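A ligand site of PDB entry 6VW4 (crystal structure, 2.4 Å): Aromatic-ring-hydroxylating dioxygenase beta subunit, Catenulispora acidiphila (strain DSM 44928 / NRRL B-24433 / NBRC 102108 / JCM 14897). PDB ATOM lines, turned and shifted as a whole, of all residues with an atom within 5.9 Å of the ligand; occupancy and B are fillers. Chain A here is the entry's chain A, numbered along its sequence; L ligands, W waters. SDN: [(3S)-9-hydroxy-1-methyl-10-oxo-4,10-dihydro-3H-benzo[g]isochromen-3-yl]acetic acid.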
ATOM      1  N   MET A  22       7.069  25.223  -8.384  1.00  0.00           N
ATOM      2  CA  MET A  22       7.565  25.165  -9.746  1.00  0.00           C
ATOM      3  C   MET A  22       7.554  26.532 -10.420  1.00  0.00           C
ATOM      4  O   MET A  22       8.355  26.763 -11.329  1.00  0.00           O
ATOM      5  CB  MET A  22       6.769  24.178 -10.609  1.00  0.00           C
ATOM      6  CG  MET A  22       6.901  22.745 -10.236  1.00  0.00           C
ATOM      7  SD  MET A  22       8.506  22.321  -9.469  1.00  0.00           S
ATOM      8  CE  MET A  22       9.267  22.015 -11.138  1.00  0.00           C
ATOM      9  N   LEU A  25      10.954  27.688  -9.374  1.00  0.00           N
ATOM     10  CA  LEU A  25      12.023  26.963 -10.071  1.00  0.00           C
ATOM     11  C   LEU A  25      12.153  27.430 -11.527  1.00  0.00           C
ATOM     12  O   LEU A  25      13.249  27.770 -11.992  1.00  0.00           O
ATOM     13  CB  LEU A  25      11.748  25.467 -10.005  1.00  0.00           C
ATOM     14  CG  LEU A  25      12.660  24.661 -10.933  1.00  0.00           C
ATOM     15  CD1 LEU A  25      14.052  24.782 -10.356  1.00  0.00           C
ATOM     16  CD2 LEU A  25      12.305  23.213 -11.078  1.00  0.00           C
ATOM     17  N   TYR A  33      12.799  28.234  -4.239  1.00  0.00           N
ATOM     18  CA  TYR A  33      12.410  26.852  -4.443  1.00  0.00           C
ATOM     19  C   TYR A  33      12.939  25.996  -3.317  1.00  0.00           C
ATOM     20  O   TYR A  33      12.208  25.150  -2.781  1.00  0.00           O
ATOM     21  CB  TYR A  33      12.900  26.333  -5.796  1.00  0.00           C
ATOM     22  CG  TYR A  33      12.758  24.835  -6.031  1.00  0.00           C
ATOM     23  CD1 TYR A  33      11.561  24.303  -6.425  1.00  0.00           C
ATOM     24  CD2 TYR A  33      13.828  23.961  -5.868  1.00  0.00           C
ATOM     25  CE1 TYR A  33      11.402  22.967  -6.672  1.00  0.00           C
ATOM     26  CE2 TYR A  33      13.676  22.599  -6.093  1.00  0.00           C
ATOM     27  CZ  TYR A  33      12.446  22.128  -6.523  1.00  0.00           C
ATOM     28  OH  TYR A  33      12.217  20.800  -6.775  1.00  0.00           O
ATOM     29  N   PHE A  43      16.241  15.864  -2.419  1.00  0.00           N
ATOM     30  CA  PHE A  43      15.882  16.114  -3.818  1.00  0.00           C
ATOM     31  C   PHE A  43      16.719  15.226  -4.729  1.00  0.00           C
ATOM     32  O   PHE A  43      17.872  15.545  -5.009  1.00  0.00           O
ATOM     33  CB  PHE A  43      16.157  17.560  -4.128  1.00  0.00           C
ATOM     34  CG  PHE A  43      15.715  18.000  -5.503  1.00  0.00           C
ATOM     35  CD1 PHE A  43      14.723  17.314  -6.201  1.00  0.00           C
ATOM     36  CD2 PHE A  43      16.275  19.137  -6.078  1.00  0.00           C
ATOM     37  CE1 PHE A  43      14.295  17.767  -7.464  1.00  0.00           C
ATOM     38  CE2 PHE A  43      15.867  19.582  -7.349  1.00  0.00           C
ATOM     39  CZ  PHE A  43      14.866  18.898  -8.032  1.00  0.00           C
ATOM     40  N   HIS A  45      16.809  14.550  -8.233  1.00  0.00           N
ATOM     41  CA  HIS A  45      16.226  15.028  -9.490  1.00  0.00           C
ATOM     42  C   HIS A  45      16.558  14.138 -10.697  1.00  0.00           C
ATOM     43  O   HIS A  45      15.845  14.179 -11.704  1.00  0.00           O
ATOM     44  CB  HIS A  45      16.675  16.486  -9.785  1.00  0.00           C
ATOM     45  CG  HIS A  45      18.111  16.625 -10.203  1.00  0.00           C
ATOM     46  ND1 HIS A  45      18.488  17.068 -11.452  1.00  0.00           N
ATOM     47  CD2 HIS A  45      19.256  16.438  -9.504  1.00  0.00           C
ATOM     48  CE1 HIS A  45      19.805  17.115 -11.519  1.00  0.00           C
ATOM     49  NE2 HIS A  45      20.302  16.743 -10.346  1.00  0.00           N
ATOM     50  N   THR A  46      17.647  13.358 -10.637  1.00  0.00           N
ATOM     51  CA  THR A  46      18.006  12.518 -11.784  1.00  0.00           C
ATOM     52  C   THR A  46      18.509  11.157 -11.330  1.00  0.00           C
ATOM     53  O   THR A  46      19.406  11.081 -10.468  1.00  0.00           O
ATOM     54  CB  THR A  46      19.052  13.186 -12.687  1.00  0.00           C
ATOM     55  OG1 THR A  46      20.180  13.622 -11.909  1.00  0.00           O
ATOM     56  CG2 THR A  46      18.442  14.379 -13.438  1.00  0.00           C
ATOM     57  N   LEU A  62      21.130  22.996  -8.485  1.00  0.00           N
ATOM     58  CA  LEU A  62      20.394  23.648  -9.560  1.00  0.00           C
ATOM     59  C   LEU A  62      21.265  24.652 -10.310  1.00  0.00           C
ATOM     60  O   LEU A  62      21.073  24.864 -11.512  1.00  0.00           O
ATOM     61  CB  LEU A  62      19.155  24.359  -9.021  1.00  0.00           C
ATOM     62  CG  LEU A  62      18.055  23.437  -8.481  1.00  0.00           C
ATOM     63  CD1 LEU A  62      17.011  24.267  -7.740  1.00  0.00           C
ATOM     64  CD2 LEU A  62      17.441  22.581  -9.582  1.00  0.00           C
ATOM     65  N   PHE A  65      23.371  22.332 -12.679  1.00  0.00           N
ATOM     66  CA  PHE A  65      22.556  21.842 -13.794  1.00  0.00           C
ATOM     67  C   PHE A  65      22.278  22.940 -14.808  1.00  0.00           C
ATOM     68  O   PHE A  65      22.330  22.696 -16.026  1.00  0.00           O
ATOM     69  CB  PHE A  65      21.246  21.255 -13.227  1.00  0.00           C
ATOM     70  CG  PHE A  65      20.268  20.793 -14.257  1.00  0.00           C
ATOM     71  CD1 PHE A  65      19.412  21.693 -14.888  1.00  0.00           C
ATOM     72  CD2 PHE A  65      20.203  19.452 -14.595  1.00  0.00           C
ATOM     73  CE1 PHE A  65      18.517  21.259 -15.847  1.00  0.00           C
ATOM     74  CE2 PHE A  65      19.318  19.011 -15.546  1.00  0.00           C
ATOM     75  CZ  PHE A  65      18.469  19.918 -16.181  1.00  0.00           C
ATOM     76  N   HIS A  66      22.008  24.163 -14.334  1.00  0.00           N
ATOM     77  CA  HIS A  66      21.591  25.234 -15.235  1.00  0.00           C
ATOM     78  C   HIS A  66      22.750  26.030 -15.873  1.00  0.00           C
ATOM     79  O   HIS A  66      22.600  26.477 -17.009  1.00  0.00           O
ATOM     80  CB  HIS A  66      20.649  26.228 -14.532  1.00  0.00           C
ATOM     81  CG  HIS A  66      19.224  25.732 -14.427  1.00  0.00           C
ATOM     82  ND1 HIS A  66      18.891  24.616 -13.686  1.00  0.00           N
ATOM     83  CD2 HIS A  66      18.063  26.187 -14.964  1.00  0.00           C
ATOM     84  CE1 HIS A  66      17.584  24.400 -13.777  1.00  0.00           C
ATOM     85  NE2 HIS A  66      17.064  25.340 -14.547  1.00  0.00           N
ATOM     86  N   ARG A  76      12.284  26.908 -19.287  1.00  0.00           N
ATOM     87  CA  ARG A  76      11.708  25.614 -18.959  1.00  0.00           C
ATOM     88  C   ARG A  76      10.391  25.782 -18.211  1.00  0.00           C
ATOM     89  O   ARG A  76      10.153  26.784 -17.542  1.00  0.00           O
ATOM     90  CB  ARG A  76      12.639  24.813 -18.076  1.00  0.00           C
ATOM     91  CG  ARG A  76      14.107  24.965 -18.378  1.00  0.00           C
ATOM     92  CD  ARG A  76      14.780  23.599 -18.479  1.00  0.00           C
ATOM     93  NE  ARG A  76      14.520  22.752 -17.308  1.00  0.00           N
ATOM     94  CZ  ARG A  76      14.743  21.449 -17.267  1.00  0.00           C
ATOM     95  NH1 ARG A  76      15.214  20.835 -18.343  1.00  0.00           N
ATOM     96  NH2 ARG A  76      14.471  20.757 -16.174  1.00  0.00           N
ATOM     97  N   HIS A  78       7.571  23.034 -16.015  1.00  0.00           N
ATOM     98  CA  HIS A  78       7.255  21.715 -15.485  1.00  0.00           C
ATOM     99  C   HIS A  78       5.758  21.644 -15.289  1.00  0.00           C
ATOM    100  O   HIS A  78       5.208  22.381 -14.455  1.00  0.00           O
ATOM    101  CB  HIS A  78       7.931  21.458 -14.148  1.00  0.00           C
ATOM    102  CG  HIS A  78       9.399  21.362 -14.249  1.00  0.00           C
ATOM    103  ND1 HIS A  78      10.208  22.461 -14.379  1.00  0.00           N
ATOM    104  CD2 HIS A  78      10.227  20.281 -14.259  1.00  0.00           C
ATOM    105  CE1 HIS A  78      11.465  22.078 -14.484  1.00  0.00           C
ATOM    106  NE2 HIS A  78      11.503  20.764 -14.389  1.00  0.00           N
ATOM    107  N   PHE A  80       2.683  19.452 -13.993  1.00  0.00           N
ATOM    108  CA  PHE A  80       2.331  18.348 -13.147  1.00  0.00           C
ATOM    109  C   PHE A  80       0.922  17.900 -13.476  1.00  0.00           C
ATOM    110  O   PHE A  80       0.033  18.733 -13.654  1.00  0.00           O
ATOM    111  CB  PHE A  80       2.435  18.779 -11.698  1.00  0.00           C
ATOM    112  CG  PHE A  80       3.837  18.950 -11.185  1.00  0.00           C
ATOM    113  CD1 PHE A  80       4.924  18.955 -12.022  1.00  0.00           C
ATOM    114  CD2 PHE A  80       4.057  19.163  -9.813  1.00  0.00           C
ATOM    115  CE1 PHE A  80       6.202  19.100 -11.510  1.00  0.00           C
ATOM    116  CE2 PHE A  80       5.327  19.315  -9.299  1.00  0.00           C
ATOM    117  CZ  PHE A  80       6.403  19.289 -10.161  1.00  0.00           C
ATOM    118  N   PHE A 100       2.738  11.543  -8.731  1.00  0.00           N
ATOM    119  CA  PHE A 100       2.224  12.301  -9.841  1.00  0.00           C
ATOM    120  C   PHE A 100       3.166  12.197 -11.030  1.00  0.00           C
ATOM    121  O   PHE A 100       4.240  11.603 -10.963  1.00  0.00           O
ATOM    122  CB  PHE A 100       2.003  13.774  -9.403  1.00  0.00           C
ATOM    123  CG  PHE A 100       3.254  14.470  -8.940  1.00  0.00           C
ATOM    124  CD1 PHE A 100       3.706  14.330  -7.612  1.00  0.00           C
ATOM    125  CD2 PHE A 100       3.983  15.234  -9.813  1.00  0.00           C
ATOM    126  CE1 PHE A 100       4.854  14.983  -7.168  1.00  0.00           C
ATOM    127  CE2 PHE A 100       5.175  15.899  -9.377  1.00  0.00           C
ATOM    128  CZ  PHE A 100       5.607  15.772  -8.064  1.00  0.00           C
ATOM    129  N   THR A 102       5.163  14.298 -14.159  1.00  0.00           N
ATOM    130  CA  THR A 102       5.717  15.554 -14.636  1.00  0.00           C
ATOM    131  C   THR A 102       6.000  15.437 -16.122  1.00  0.00           C
ATOM    132  O   THR A 102       6.469  14.397 -16.587  1.00  0.00           O
ATOM    133  CB  THR A 102       7.028  15.935 -13.925  1.00  0.00           C
ATOM    134  OG1 THR A 102       6.781  16.025 -12.536  1.00  0.00           O
ATOM    135  CG2 THR A 102       7.491  17.305 -14.421  1.00  0.00           C
ATOM    136  N   VAL A 104       8.261  17.834 -18.750  1.00  0.00           N
ATOM    137  CA  VAL A 104       9.190  18.948 -18.907  1.00  0.00           C
ATOM    138  C   VAL A 104       9.088  19.549 -20.296  1.00  0.00           C
ATOM    139  O   VAL A 104       9.092  18.840 -21.303  1.00  0.00           O
ATOM    140  CB  VAL A 104      10.623  18.487 -18.609  1.00  0.00           C
ATOM    141  CG1 VAL A 104      11.573  19.676 -18.609  1.00  0.00           C
ATOM    142  CG2 VAL A 104      10.665  17.744 -17.289  1.00  0.00           C
ATOM    143  N   GLY A 115       9.893  16.953 -23.272  1.00  0.00           N
ATOM    144  CA  GLY A 115      10.296  15.743 -22.577  1.00  0.00           C
ATOM    145  C   GLY A 115      11.472  16.062 -21.697  1.00  0.00           C
ATOM    146  O   GLY A 115      12.004  17.170 -21.738  1.00  0.00           O
ATOM    147  N   PRO A 116      11.853  15.138 -20.818  1.00  0.00           N
ATOM    148  CA  PRO A 116      11.116  13.869 -20.667  1.00  0.00           C
ATOM    149  C   PRO A 116       9.822  13.908 -19.861  1.00  0.00           C
ATOM    150  O   PRO A 116       9.417  14.910 -19.287  1.00  0.00           O
ATOM    151  CB  PRO A 116      12.104  12.973 -19.916  1.00  0.00           C
ATOM    152  CG  PRO A 116      12.849  13.983 -18.992  1.00  0.00           C
ATOM    153  CD  PRO A 116      12.985  15.258 -19.878  1.00  0.00           C
ATOM    154  N   CYS A 118       8.173  12.165 -16.586  1.00  0.00           N
ATOM    155  CA  CYS A 118       8.755  11.737 -15.322  1.00  0.00           C
ATOM    156  C   CYS A 118       7.732  11.419 -14.227  1.00  0.00           C
ATOM    157  O   CYS A 118       6.996  12.314 -13.780  1.00  0.00           O
ATOM    158  CB  CYS A 118       9.686  12.815 -14.750  1.00  0.00           C
ATOM    159  SG  CYS A 118      11.036  13.398 -15.777  1.00  0.00           S
ATOM    160  N   VAL A 120       7.000  10.973 -10.399  1.00  0.00           N
ATOM    161  CA  VAL A 120       7.649  11.611  -9.267  1.00  0.00           C
ATOM    162  C   VAL A 120       6.901  11.220  -8.004  1.00  0.00           C
ATOM    163  O   VAL A 120       5.669  11.179  -7.993  1.00  0.00           O
ATOM    164  CB  VAL A 120       7.673  13.147  -9.399  1.00  0.00           C
ATOM    165  CG1 VAL A 120       8.418  13.784  -8.196  1.00  0.00           C
ATOM    166  CG2 VAL A 120       8.317  13.550 -10.697  1.00  0.00           C
ATOM    167  N   ARG A 137      11.602  14.651  -2.615  1.00  0.00           N
ATOM    168  CA  ARG A 137      11.172  14.569  -4.004  1.00  0.00           C
ATOM    169  C   ARG A 137      12.080  13.579  -4.737  1.00  0.00           C
ATOM    170  O   ARG A 137      13.304  13.758  -4.793  1.00  0.00           O
ATOM    171  CB  ARG A 137      11.202  15.943  -4.673  1.00  0.00           C
ATOM    172  CG  ARG A 137      11.064  15.888  -6.193  1.00  0.00           C
ATOM    173  CD  ARG A 137      10.614  17.219  -6.720  1.00  0.00           C
ATOM    174  NE  ARG A 137       9.230  17.452  -6.331  1.00  0.00           N
ATOM    175  CZ  ARG A 137       8.612  18.612  -6.458  1.00  0.00           C
ATOM    176  NH1 ARG A 137       9.260  19.658  -6.950  1.00  0.00           N
ATOM    177  NH2 ARG A 137       7.353  18.751  -6.065  1.00  0.00           N
ATOM    178  N   VAL A 139      12.525  11.772  -8.282  1.00  0.00           N
ATOM    179  CA  VAL A 139      12.171  11.828  -9.695  1.00  0.00           C
ATOM    180  C   VAL A 139      12.715  10.605 -10.420  1.00  0.00           C
ATOM    181  O   VAL A 139      13.905  10.290 -10.321  1.00  0.00           O
ATOM    182  CB  VAL A 139      12.712  13.114 -10.344  1.00  0.00           C
ATOM    183  CG1 VAL A 139      12.214  13.190 -11.798  1.00  0.00           C
ATOM    184  CG2 VAL A 139      12.272  14.324  -9.584  1.00  0.00           C
ATOM    185  N   HIS A 141      12.905   9.068 -14.563  1.00  0.00           N
ATOM    186  CA  HIS A 141      12.900   9.525 -15.953  1.00  0.00           C
ATOM    187  C   HIS A 141      12.430   8.378 -16.832  1.00  0.00           C
ATOM    188  O   HIS A 141      13.055   7.324 -16.839  1.00  0.00           O
ATOM    189  CB  HIS A 141      14.283   9.965 -16.425  1.00  0.00           C
ATOM    190  CG  HIS A 141      14.746  11.255 -15.841  1.00  0.00           C
ATOM    191  ND1 HIS A 141      14.111  11.864 -14.775  1.00  0.00           N
ATOM    192  CD2 HIS A 141      15.773  12.068 -16.179  1.00  0.00           C
ATOM    193  CE1 HIS A 141      14.736  12.988 -14.487  1.00  0.00           C
ATOM    194  NE2 HIS A 141      15.740  13.137 -15.328  1.00  0.00           N
HETATM  195  O4  SDN L   1      12.012  19.980  -9.495  1.00  0.00           O
HETATM  196  C11 SDN L   1      11.387  18.957 -10.206  1.00  0.00           C
HETATM  197  C12 SDN L   1      11.995  18.358 -11.305  1.00  0.00           C
HETATM  198  C13 SDN L   1      13.404  18.838 -11.738  1.00  0.00           C
HETATM  199  O5  SDN L   1      13.943  19.708 -11.139  1.00  0.00           O
HETATM  200  C14 SDN L   1      14.072  18.183 -12.942  1.00  0.00           C
HETATM  201  C15 SDN L   1      15.478  18.643 -13.360  1.00  0.00           C
HETATM  202  O3  SDN L   1      16.291  17.650 -14.023  1.00  0.00           O
HETATM  203  C16 SDN L   1      16.090  19.995 -12.951  1.00  0.00           C
HETATM  204  C10 SDN L   1      10.115  18.558  -9.848  1.00  0.00           C
HETATM  205  C9  SDN L   1       9.448  17.550 -10.554  1.00  0.00           C
HETATM  206  C8  SDN L   1      10.059  16.939 -11.643  1.00  0.00           C
HETATM  207  C7  SDN L   1      11.327  17.341 -12.032  1.00  0.00           C
HETATM  208  C6  SDN L   1      11.997  16.654 -13.266  1.00  0.00           C
HETATM  209  C5  SDN L   1      13.397  17.131 -13.662  1.00  0.00           C
HETATM  210  C4  SDN L   1      14.062  16.498 -14.802  1.00  0.00           C
HETATM  211  C3  SDN L   1      15.546  16.788 -14.952  1.00  0.00           C
HETATM  212  C2  SDN L   1      15.508  17.547 -16.264  1.00  0.00           C
HETATM  213  C1  SDN L   1      16.090  16.937 -17.525  1.00  0.00           C
HETATM  214  O2  SDN L   1      16.549  15.775 -17.508  1.00  0.00           O
HETATM  215  O1  SDN L   1      16.103  17.639 -18.581  1.00  0.00           O
HETATM  216  O   HOH W   1      14.858  22.897 -14.308  1.00  0.00           O
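The side-chain hydroxyl of Tyr 33 lies within hydrogen-bond range of an oxygen (O4) of the ligand, 2.8 Å away. The guanidinium group (NH1) of Arg 76 is in salt-bridge range of an oxygen (O1) of the ligand. O3 of the ligand is in hydrogen-bond range of ND1 of His 45 (3.4 Å).
OH of Tyr 33 is in hydrogen-bond range of NH1 of Arg 137 (3.2 Å). The guanidinium group (NH1) of Arg 137 is in hydrogen-bond range of the side-chain sulfur (SD) of Met 22, at 3.7 Å. NH2 of Arg 76 is in hydrogen-bond range of NE2 of His 78, 3.5 Å away. NE2 of His 45 sits at hydrogen-bond distance from OG1 of Thr 46. A ring nitrogen (ND1) of His 141 is in hydrogen-bond range of the side-chain sulfur (SG) of Cys 118, 3.6 Å away. The backbone NH of Thr 102 is in hydrogen-bond range of the backbone carbonyl oxygen of Cys 118, at 2.7 Å. O of Phe 100 lies within hydrogen-bond range of N of Val 120 (2.9 Å).
CE of Met 22 touches C10 of the ligand (3.8 Å). Leu 25 touches the ligand. Phe 43 touches the ligand (CZ to O5, 3.3 Å). CG2 of Thr 46 touches O3 of the ligand, 3.96 Å away. Phe 65 touches the ligand (CE2 to O3, 3.7 Å). His 78 touches the ligand. CZ of Phe 80 touches C9 of the ligand, at 3.5 Å. OG1 of Thr 102 touches C8 of the ligand, at 3.5 Å. Val 120 touches the ligand. NH1 of Arg 137 touches C10 of the ligand (3.2 Å). CG1 of Val 139 touches C6 of the ligand (3.8 Å). His 141 touches the ligand. Hydrophobic or aromatic side chains that line the ligand: Met 22, Leu 25, Tyr 33, Phe 43, Phe 65, His 78, Phe 80, Val 120, Val 139 and His 141. Within 4 Å of the ligand: Met 22, Leu 25, Tyr 33, Phe 43, His 45, Thr 46, Phe 65, Arg 76, His 78, Phe 80, Thr 102, Val 120, Arg 137, Val 139 and His 141. The nearest printed residue that does not touch the ligand is Pro 116 (4.1 Å).
Water W1 lies within hydrogen-bond range of NH2 of Arg 76 and NE2 of His 66.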
